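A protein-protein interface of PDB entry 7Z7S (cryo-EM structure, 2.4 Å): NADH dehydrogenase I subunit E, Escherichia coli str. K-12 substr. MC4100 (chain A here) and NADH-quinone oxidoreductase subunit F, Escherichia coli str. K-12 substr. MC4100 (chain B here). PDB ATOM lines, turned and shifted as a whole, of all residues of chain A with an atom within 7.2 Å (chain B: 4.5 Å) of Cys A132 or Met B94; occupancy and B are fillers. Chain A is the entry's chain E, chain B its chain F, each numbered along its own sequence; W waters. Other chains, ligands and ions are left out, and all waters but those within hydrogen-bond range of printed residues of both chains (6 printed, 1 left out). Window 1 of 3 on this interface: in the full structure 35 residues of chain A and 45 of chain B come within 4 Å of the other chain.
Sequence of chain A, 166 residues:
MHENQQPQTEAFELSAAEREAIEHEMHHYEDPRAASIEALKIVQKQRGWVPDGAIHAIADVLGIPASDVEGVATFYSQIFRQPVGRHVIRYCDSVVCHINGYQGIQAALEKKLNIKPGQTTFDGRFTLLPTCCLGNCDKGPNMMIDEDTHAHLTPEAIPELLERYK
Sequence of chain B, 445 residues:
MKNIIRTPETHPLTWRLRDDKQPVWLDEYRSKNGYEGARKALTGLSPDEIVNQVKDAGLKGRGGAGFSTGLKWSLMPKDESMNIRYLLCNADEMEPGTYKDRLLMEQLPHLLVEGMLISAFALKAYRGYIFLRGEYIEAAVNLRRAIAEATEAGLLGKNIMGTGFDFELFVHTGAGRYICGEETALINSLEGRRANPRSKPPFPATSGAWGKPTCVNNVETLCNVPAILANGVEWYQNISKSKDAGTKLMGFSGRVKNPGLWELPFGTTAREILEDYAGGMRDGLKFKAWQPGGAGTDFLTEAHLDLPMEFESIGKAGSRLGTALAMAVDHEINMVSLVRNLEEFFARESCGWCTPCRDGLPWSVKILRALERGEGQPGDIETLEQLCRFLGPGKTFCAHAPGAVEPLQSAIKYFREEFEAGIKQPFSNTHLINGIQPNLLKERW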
ATOM      1  N   SER A  77     -12.697 -25.455  26.187  1.00  0.00           N
ATOM      2  CA  SER A  77     -11.654 -26.469  26.168  1.00  0.00           C
ATOM      3  C   SER A  77     -11.609 -27.280  27.457  1.00  0.00           C
ATOM      4  O   SER A  77     -11.190 -28.439  27.434  1.00  0.00           O
ATOM      5  CB  SER A  77     -10.300 -25.817  25.899  1.00  0.00           C
ATOM      6  OG  SER A  77     -10.044 -24.771  26.810  1.00  0.00           O
ATOM      7  N   GLN A  78     -12.044 -26.712  28.575  1.00  0.00           N
ATOM      8  CA  GLN A  78     -11.969 -27.426  29.841  1.00  0.00           C
ATOM      9  C   GLN A  78     -13.204 -28.258  30.136  1.00  0.00           C
ATOM     10  O   GLN A  78     -13.273 -28.873  31.203  1.00  0.00           O
ATOM     11  CB  GLN A  78     -11.719 -26.454  30.993  1.00  0.00           C
ATOM     12  CG  GLN A  78     -10.472 -25.614  30.829  1.00  0.00           C
ATOM     13  CD  GLN A  78      -9.285 -26.409  30.334  1.00  0.00           C
ATOM     14  OE1 GLN A  78      -8.932 -27.443  30.896  1.00  0.00           O
ATOM     15  NE2 GLN A  78      -8.653 -25.922  29.277  1.00  0.00           N
ATOM     16  N   ARG A  90      -2.080 -30.379  33.026  1.00  0.00           N
ATOM     17  CA  ARG A  90      -2.239 -29.297  32.063  1.00  0.00           C
ATOM     18  C   ARG A  90      -0.984 -28.439  32.115  1.00  0.00           C
ATOM     19  O   ARG A  90      -0.859 -27.565  32.973  1.00  0.00           O
ATOM     20  CB  ARG A  90      -3.489 -28.482  32.352  1.00  0.00           C
ATOM     21  CG  ARG A  90      -4.737 -29.102  31.782  1.00  0.00           C
ATOM     22  CD  ARG A  90      -5.889 -28.141  31.803  1.00  0.00           C
ATOM     23  NE  ARG A  90      -6.099 -27.567  33.123  1.00  0.00           N
ATOM     24  CZ  ARG A  90      -7.016 -27.989  33.979  1.00  0.00           C
ATOM     25  NH1 ARG A  90      -7.829 -28.989  33.681  1.00  0.00           N
ATOM     26  NH2 ARG A  90      -7.116 -27.399  35.166  1.00  0.00           N
ATOM     27  N   TYR A  91      -0.060 -28.686  31.198  1.00  0.00           N
ATOM     28  CA  TYR A  91       1.172 -27.913  31.159  1.00  0.00           C
ATOM     29  C   TYR A  91       0.989 -26.706  30.253  1.00  0.00           C
ATOM     30  O   TYR A  91       0.391 -26.805  29.181  1.00  0.00           O
ATOM     31  CB  TYR A  91       2.356 -28.772  30.698  1.00  0.00           C
ATOM     32  CG  TYR A  91       2.311 -29.223  29.257  1.00  0.00           C
ATOM     33  CD1 TYR A  91       1.633 -30.376  28.896  1.00  0.00           C
ATOM     34  CD2 TYR A  91       2.953 -28.503  28.259  1.00  0.00           C
ATOM     35  CE1 TYR A  91       1.588 -30.792  27.590  1.00  0.00           C
ATOM     36  CE2 TYR A  91       2.905 -28.909  26.951  1.00  0.00           C
ATOM     37  CZ  TYR A  91       2.223 -30.056  26.622  1.00  0.00           C
ATOM     38  OH  TYR A  91       2.178 -30.469  25.316  1.00  0.00           O
ATOM     39  N   CYS A  92       1.487 -25.561  30.700  1.00  0.00           N
ATOM     40  CA  CYS A  92       1.375 -24.338  29.923  1.00  0.00           C
ATOM     41  C   CYS A  92       2.369 -24.352  28.772  1.00  0.00           C
ATOM     42  O   CYS A  92       3.558 -24.609  28.973  1.00  0.00           O
ATOM     43  CB  CYS A  92       1.619 -23.124  30.812  1.00  0.00           C
ATOM     44  SG  CYS A  92       1.760 -21.594  29.901  1.00  0.00           S
ATOM     45  N   ASP A  93       1.886 -24.066  27.564  1.00  0.00           N
ATOM     46  CA  ASP A  93       2.743 -24.011  26.389  1.00  0.00           C
ATOM     47  C   ASP A  93       2.776 -22.615  25.776  1.00  0.00           C
ATOM     48  O   ASP A  93       3.045 -22.461  24.587  1.00  0.00           O
ATOM     49  CB  ASP A  93       2.329 -25.062  25.354  1.00  0.00           C
ATOM     50  CG  ASP A  93       0.948 -24.830  24.755  1.00  0.00           C
ATOM     51  OD1 ASP A  93       0.174 -23.991  25.247  1.00  0.00           O
ATOM     52  OD2 ASP A  93       0.631 -25.516  23.766  1.00  0.00           O
ATOM     53  N   SER A  94       2.513 -21.591  26.576  1.00  0.00           N
ATOM     54  CA  SER A  94       2.443 -20.227  26.081  1.00  0.00           C
ATOM     55  C   SER A  94       3.829 -19.585  26.106  1.00  0.00           C
ATOM     56  O   SER A  94       4.829 -20.233  26.413  1.00  0.00           O
ATOM     57  CB  SER A  94       1.415 -19.436  26.879  1.00  0.00           C
ATOM     58  OG  SER A  94       0.106 -19.788  26.486  1.00  0.00           O
ATOM     59  N   PRO A 130      -1.733 -29.941  26.795  1.00  0.00           N
ATOM     60  CA  PRO A 130      -1.270 -28.558  26.769  1.00  0.00           C
ATOM     61  C   PRO A 130      -2.413 -27.626  27.113  1.00  0.00           C
ATOM     62  O   PRO A 130      -3.581 -27.908  26.842  1.00  0.00           O
ATOM     63  CB  PRO A 130      -0.809 -28.365  25.324  1.00  0.00           C
ATOM     64  CG  PRO A 130      -1.661 -29.299  24.550  1.00  0.00           C
ATOM     65  CD  PRO A 130      -1.917 -30.486  25.441  1.00  0.00           C
ATOM     66  N   THR A 131      -2.068 -26.507  27.727  1.00  0.00           N
ATOM     67  CA  THR A 131      -3.045 -25.487  28.039  1.00  0.00           C
ATOM     68  C   THR A 131      -2.428 -24.136  27.742  1.00  0.00           C
ATOM     69  O   THR A 131      -1.207 -23.987  27.686  1.00  0.00           O
ATOM     70  CB  THR A 131      -3.515 -25.557  29.501  1.00  0.00           C
ATOM     71  OG1 THR A 131      -4.524 -24.567  29.725  1.00  0.00           O
ATOM     72  CG2 THR A 131      -2.369 -25.319  30.460  1.00  0.00           C
ATOM     73  N   CYS A 132      -3.291 -23.140  27.574  1.00  0.00           N
ATOM     74  CA  CYS A 132      -2.835 -21.774  27.402  1.00  0.00           C
ATOM     75  C   CYS A 132      -2.247 -21.262  28.715  1.00  0.00           C
ATOM     76  O   CYS A 132      -2.180 -21.977  29.718  1.00  0.00           O
ATOM     77  CB  CYS A 132      -3.986 -20.889  26.931  1.00  0.00           C
ATOM     78  SG  CYS A 132      -5.574 -21.294  27.673  1.00  0.00           S
ATOM     79  N   CYS A 133      -1.825 -20.001  28.699  1.00  0.00           N
ATOM     80  CA  CYS A 133      -1.112 -19.413  29.824  1.00  0.00           C
ATOM     81  C   CYS A 133      -1.941 -19.461  31.099  1.00  0.00           C
ATOM     82  O   CYS A 133      -3.112 -19.077  31.110  1.00  0.00           O
ATOM     83  CB  CYS A 133      -0.741 -17.974  29.493  1.00  0.00           C
ATOM     84  SG  CYS A 133      -0.427 -16.921  30.903  1.00  0.00           S
ATOM     85  N   LEU A 134      -1.328 -19.951  32.169  1.00  0.00           N
ATOM     86  CA  LEU A 134      -2.004 -20.166  33.435  1.00  0.00           C
ATOM     87  C   LEU A 134      -1.984 -18.937  34.326  1.00  0.00           C
ATOM     88  O   LEU A 134      -2.387 -19.027  35.488  1.00  0.00           O
ATOM     89  CB  LEU A 134      -1.379 -21.355  34.170  1.00  0.00           C
ATOM     90  CG  LEU A 134      -1.614 -22.719  33.524  1.00  0.00           C
ATOM     91  CD1 LEU A 134      -0.711 -23.780  34.117  1.00  0.00           C
ATOM     92  CD2 LEU A 134      -3.065 -23.121  33.658  1.00  0.00           C
ATOM     93  N   GLY A 135      -1.529 -17.802  33.811  1.00  0.00           N
ATOM     94  CA  GLY A 135      -1.458 -16.583  34.592  1.00  0.00           C
ATOM     95  C   GLY A 135      -0.467 -16.651  35.730  1.00  0.00           C
ATOM     96  O   GLY A 135      -0.720 -16.097  36.803  1.00  0.00           O
ATOM     97  N   ASP B  92     -11.105 -12.693  33.687  1.00  0.00           N
ATOM     98  CA  ASP B  92     -10.689 -13.767  32.794  1.00  0.00           C
ATOM     99  C   ASP B  92      -9.173 -13.890  32.752  1.00  0.00           C
ATOM    100  O   ASP B  92      -8.626 -14.928  33.124  1.00  0.00           O
ATOM    101  CB  ASP B  92     -11.252 -13.541  31.396  1.00  0.00           C
ATOM    102  CG  ASP B  92     -11.443 -14.834  30.633  1.00  0.00           C
ATOM    103  OD1 ASP B  92     -12.148 -15.730  31.134  1.00  0.00           O
ATOM    104  OD2 ASP B  92     -10.865 -14.963  29.538  1.00  0.00           O
ATOM    105  N   GLU B  93      -8.483 -12.837  32.309  1.00  0.00           N
ATOM    106  CA  GLU B  93      -7.021 -12.715  32.323  1.00  0.00           C
ATOM    107  C   GLU B  93      -6.331 -13.926  31.686  1.00  0.00           C
ATOM    108  O   GLU B  93      -5.675 -14.727  32.348  1.00  0.00           O
ATOM    109  CB  GLU B  93      -6.491 -12.488  33.739  1.00  0.00           C
ATOM    110  CG  GLU B  93      -5.144 -11.785  33.734  1.00  0.00           C
ATOM    111  CD  GLU B  93      -4.364 -11.955  35.013  1.00  0.00           C
ATOM    112  OE1 GLU B  93      -4.317 -13.078  35.550  1.00  0.00           O
ATOM    113  OE2 GLU B  93      -3.793 -10.955  35.483  1.00  0.00           O
ATOM    114  N   MET B  94      -6.535 -14.065  30.384  1.00  0.00           N
ATOM    115  CA  MET B  94      -5.986 -15.195  29.656  1.00  0.00           C
ATOM    116  C   MET B  94      -4.865 -14.796  28.709  1.00  0.00           C
ATOM    117  O   MET B  94      -4.370 -15.646  27.966  1.00  0.00           O
ATOM    118  CB  MET B  94      -7.097 -15.913  28.894  1.00  0.00           C
ATOM    119  CG  MET B  94      -7.812 -16.970  29.702  1.00  0.00           C
ATOM    120  SD  MET B  94      -7.342 -18.627  29.213  1.00  0.00           S
ATOM    121  CE  MET B  94      -8.570 -19.577  30.087  1.00  0.00           C
ATOM    122  N   GLU B  95      -4.449 -13.539  28.724  1.00  0.00           N
ATOM    123  CA  GLU B  95      -3.349 -13.112  27.872  1.00  0.00           C
ATOM    124  C   GLU B  95      -2.041 -13.698  28.380  1.00  0.00           C
ATOM    125  O   GLU B  95      -1.746 -13.593  29.574  1.00  0.00           O
ATOM    126  CB  GLU B  95      -3.242 -11.597  27.834  1.00  0.00           C
ATOM    127  CG  GLU B  95      -2.147 -11.060  26.930  1.00  0.00           C
ATOM    128  CD  GLU B  95      -2.624 -10.765  25.523  1.00  0.00           C
ATOM    129  OE1 GLU B  95      -3.295 -11.623  24.925  1.00  0.00           O
ATOM    130  OE2 GLU B  95      -2.326  -9.671  25.010  1.00  0.00           O
ATOM    131  N   PRO B  96      -1.252 -14.333  27.521  1.00  0.00           N
ATOM    132  CA  PRO B  96       0.059 -14.828  27.946  1.00  0.00           C
ATOM    133  C   PRO B  96       0.984 -13.688  28.340  1.00  0.00           C
ATOM    134  O   PRO B  96       1.152 -12.717  27.604  1.00  0.00           O
ATOM    135  CB  PRO B  96       0.564 -15.579  26.714  1.00  0.00           C
ATOM    136  CG  PRO B  96      -0.674 -15.955  25.978  1.00  0.00           C
ATOM    137  CD  PRO B  96      -1.627 -14.832  26.192  1.00  0.00           C
ATOM    138  N   ARG B 133     -11.738 -16.849  35.525  1.00  0.00           N
ATOM    139  CA  ARG B 133     -11.266 -18.014  34.791  1.00  0.00           C
ATOM    140  C   ARG B 133     -11.215 -19.238  35.700  1.00  0.00           C
ATOM    141  O   ARG B 133     -11.014 -19.135  36.912  1.00  0.00           O
ATOM    142  CB  ARG B 133      -9.896 -17.743  34.167  1.00  0.00           C
ATOM    143  CG  ARG B 133      -8.751 -17.670  35.150  1.00  0.00           C
ATOM    144  CD  ARG B 133      -7.412 -17.461  34.471  1.00  0.00           C
ATOM    145  NE  ARG B 133      -6.992 -18.579  33.637  1.00  0.00           N
ATOM    146  CZ  ARG B 133      -5.883 -18.587  32.914  1.00  0.00           C
ATOM    147  NH1 ARG B 133      -5.073 -17.545  32.879  1.00  0.00           N
ATOM    148  NH2 ARG B 133      -5.574 -19.672  32.214  1.00  0.00           N
ATOM    149  N   GLU B 135      -9.119 -21.644  35.996  1.00  0.00           N
ATOM    150  CA  GLU B 135      -7.823 -22.055  36.510  1.00  0.00           C
ATOM    151  C   GLU B 135      -7.417 -21.302  37.766  1.00  0.00           C
ATOM    152  O   GLU B 135      -6.408 -21.658  38.379  1.00  0.00           O
ATOM    153  CB  GLU B 135      -6.756 -21.871  35.429  1.00  0.00           C
ATOM    154  CG  GLU B 135      -6.984 -22.718  34.195  1.00  0.00           C
ATOM    155  CD  GLU B 135      -7.826 -22.018  33.145  1.00  0.00           C
ATOM    156  OE1 GLU B 135      -8.314 -20.905  33.413  1.00  0.00           O
ATOM    157  OE2 GLU B 135      -8.007 -22.587  32.052  1.00  0.00           O
ATOM    158  N   GLY B 176     -12.428 -22.133  30.302  1.00  0.00           N
ATOM    159  CA  GLY B 176     -11.172 -22.162  29.583  1.00  0.00           C
ATOM    160  C   GLY B 176     -11.164 -21.818  28.110  1.00  0.00           C
ATOM    161  O   GLY B 176     -10.858 -22.678  27.282  1.00  0.00           O
ATOM    162  N   ARG B 177     -11.495 -20.579  27.763  1.00  0.00           N
ATOM    163  CA  ARG B 177     -11.209 -20.055  26.435  1.00  0.00           C
ATOM    164  C   ARG B 177     -10.734 -18.620  26.575  1.00  0.00           C
ATOM    165  O   ARG B 177     -11.274 -17.856  27.376  1.00  0.00           O
ATOM    166  CB  ARG B 177     -12.426 -20.114  25.505  1.00  0.00           C
ATOM    167  CG  ARG B 177     -12.670 -21.463  24.860  1.00  0.00           C
ATOM    168  CD  ARG B 177     -11.609 -21.829  23.842  1.00  0.00           C
ATOM    169  NE  ARG B 177     -11.904 -23.118  23.230  1.00  0.00           N
ATOM    170  CZ  ARG B 177     -11.010 -23.902  22.645  1.00  0.00           C
ATOM    171  NH1 ARG B 177      -9.738 -23.559  22.562  1.00  0.00           N
ATOM    172  NH2 ARG B 177     -11.405 -25.061  22.131  1.00  0.00           N
ATOM    173  N   TYR B 178      -9.725 -18.263  25.787  1.00  0.00           N
ATOM    174  CA  TYR B 178      -9.132 -16.935  25.873  1.00  0.00           C
ATOM    175  C   TYR B 178     -10.069 -15.857  25.345  1.00  0.00           C
ATOM    176  O   TYR B 178     -10.034 -14.721  25.827  1.00  0.00           O
ATOM    177  CB  TYR B 178      -7.805 -16.947  25.119  1.00  0.00           C
ATOM    178  CG  TYR B 178      -7.249 -15.620  24.683  1.00  0.00           C
ATOM    179  CD1 TYR B 178      -6.500 -14.842  25.547  1.00  0.00           C
ATOM    180  CD2 TYR B 178      -7.424 -15.172  23.390  1.00  0.00           C
ATOM    181  CE1 TYR B 178      -5.970 -13.645  25.142  1.00  0.00           C
ATOM    182  CE2 TYR B 178      -6.902 -13.978  22.984  1.00  0.00           C
ATOM    183  CZ  TYR B 178      -6.175 -13.220  23.856  1.00  0.00           C
ATOM    184  OH  TYR B 178      -5.657 -12.031  23.422  1.00  0.00           O
ATOM    185  N   PHE B 345      -0.824 -20.243  19.764  1.00  0.00           N
ATOM    186  CA  PHE B 345      -1.791 -19.844  20.781  1.00  0.00           C
ATOM    187  C   PHE B 345      -2.944 -19.059  20.167  1.00  0.00           C
ATOM    188  O   PHE B 345      -4.113 -19.342  20.435  1.00  0.00           O
ATOM    189  CB  PHE B 345      -1.112 -19.012  21.869  1.00  0.00           C
ATOM    190  CG  PHE B 345      -2.072 -18.232  22.717  1.00  0.00           C
ATOM    191  CD1 PHE B 345      -2.786 -18.859  23.719  1.00  0.00           C
ATOM    192  CD2 PHE B 345      -2.277 -16.876  22.505  1.00  0.00           C
ATOM    193  CE1 PHE B 345      -3.673 -18.154  24.495  1.00  0.00           C
ATOM    194  CE2 PHE B 345      -3.181 -16.175  23.271  1.00  0.00           C
ATOM    195  CZ  PHE B 345      -3.875 -16.814  24.265  1.00  0.00           C
ATOM    196  N   ARG B 348      -5.253 -21.196  17.810  1.00  0.00           N
ATOM    197  CA  ARG B 348      -6.109 -22.153  18.492  1.00  0.00           C
ATOM    198  C   ARG B 348      -7.070 -21.499  19.476  1.00  0.00           C
ATOM    199  O   ARG B 348      -7.975 -22.174  19.970  1.00  0.00           O
ATOM    200  CB  ARG B 348      -5.257 -23.209  19.191  1.00  0.00           C
ATOM    201  CG  ARG B 348      -4.781 -22.849  20.568  1.00  0.00           C
ATOM    202  CD  ARG B 348      -3.881 -23.942  21.086  1.00  0.00           C
ATOM    203  NE  ARG B 348      -3.508 -23.738  22.478  1.00  0.00           N
ATOM    204  CZ  ARG B 348      -2.528 -24.388  23.084  1.00  0.00           C
ATOM    205  NH1 ARG B 348      -1.777 -25.262  22.436  1.00  0.00           N
ATOM    206  NH2 ARG B 348      -2.300 -24.161  24.371  1.00  0.00           N
HETATM  207  O   HOH W   1      -7.960 -22.737  29.170  1.00  0.00           O
HETATM  208  O   HOH W   2      -6.614 -24.951  31.747  1.00  0.00           O
HETATM  209  O   HOH W   3      -5.371 -23.015  24.299  1.00  0.00           O
HETATM  210  O   HOH W   4      -0.477 -21.559  24.365  1.00  0.00           O
HETATM  211  O   HOH W   5      -5.353 -21.822  30.330  1.00  0.00           O
HETATM  212  O   HOH W   6      -8.322 -22.671  26.075  1.00  0.00           O
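Water W4 lies within hydrogen-bond range of the side-chain carboxylate (OD1) of Asp A93 (2.7 Å), the side-chain hydroxyl (OG) of Ser A94 (2.8 Å) and the guanidinium group (NH2) of Arg B348 (3.2 Å).
Water W3 lies within hydrogen-bond range of NE of Arg B348 and SG of Cys A132.
Water W5 lies within hydrogen-bond range of SG of Cys A132 (2.7 Å), NH2 of Arg B133 (2.9 Å), OG1 of Thr A131 (2.9 Å) and OE2 of Glu B135 (3.3 Å).
Water W2 lies within hydrogen-bond range of the side-chain carboxylate (OE2) of Glu B135, the side-chain hydroxyl (OG1) of Thr A131, the guanidinium group (NE) of Arg A90 and the side-chain amide nitrogen (NE2) of Gln A78.
Water W6 lies within hydrogen-bond range of O of Gly B176 (2.8 Å), OG of Ser A77 (2.8 Å) and SG of Cys A132 (3.5 Å).
Water W1 lies within hydrogen-bond range of the side-chain carboxylate (OE2) of Glu B135 (2.9 Å), the side-chain sulfur (SG) of Cys A132 (3.2 Å), the side-chain amide nitrogen (NE2) of Gln A78 (3.3 Å) and the backbone carbonyl oxygen (O) of Gly B176 (3.5 Å).
The side-chain sulfur (SD) of Met B94 sits at hydrogen-bond distance from the guanidinium group (NH2) of Arg B133 (3.6 Å).
NE of Arg B133 is in salt-bridge range of OE1 of Glu B135, 2.7 Å away.
The guanidinium group of Arg B177 lies within hydrogen-bond range of the backbone carbonyl oxygen of Arg B348, 3.4 Å away.
OE1 of Gln A78 lies close to NH1 of Arg A90 (3.4 Å).
N of Asp A93 is in hydrogen-bond range of O of Thr A131, at 3.1 Å.
The side-chain hydroxyl (OG) of Ser A94 is in hydrogen-bond range of the backbone NH (N) of Cys A133, at 2.9 Å.
SG of Cys A132 lies within hydrogen-bond range of SD of Met B94 (3.6 Å).
The guanidinium group (NH2) of Arg B133 is in hydrogen-bond range of the backbone carbonyl oxygen (O) of Cys A133 (2.8 Å).
OD1 of Asp A93 lies within salt-bridge range of NH2 of Arg B348.
The guanidinium group (NH2) of Arg B348 lies close to the backbone carbonyl oxygen (O) of Thr A131 (3.5 Å).
OG of Ser A77 lies close to O of Gly B176 (2.3 Å).
Printed residues of chain B within 4 Å of Leu A134: Arg B133 and Glu B135.
Of chain A, only Cys A132 comes within 4 Å of Met B94.
Printed residues of chain A within 4 Å of Pro B96: Ser A94 (3.9 Å) and Cys A133 (3.6 Å).
Of the printed residues of chain A, Arg B133 touches Cys A133 (2.8 Å), Leu A134 (3.7 Å) and Gly A135 (3.7 Å).
Printed residues of chain A within 4 Å of Arg B177: Ser A77.
The nearest printed residue of chain B that does not touch Cys A132 is Arg B133 (4.8 Å).
The nearest residue of chain A that does not touch Met B94 is Cys A133 (4.6 Å).
The nearest printed residue of chain B that does not touch Ser A77 is Glu B135 (6.0 Å).
Of the 13 printed residues of chain A, 9 touch a printed residue of chain B.
Hydrophobic or aromatic side chains of chain A within 4 Å of the printed part of chain B: Leu A134.
Of the 12 printed residues of chain B, 9 touch a printed residue of chain A.
Among the printed residues, 15 pairs touch across the chains.
Among the printed residues, merely in contact across the chains: Ser A77 with Arg B177, Gln A78 with Gly B176, Ser A94 with Pro B96, Cys A132 with Phe B345, Cys A132 with Arg B348, Cys A133 with Glu B95, Cys A133 with Pro B96, Leu A134 with Arg B133, Leu A134 with Glu B135 and Gly A135 with Arg B133.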
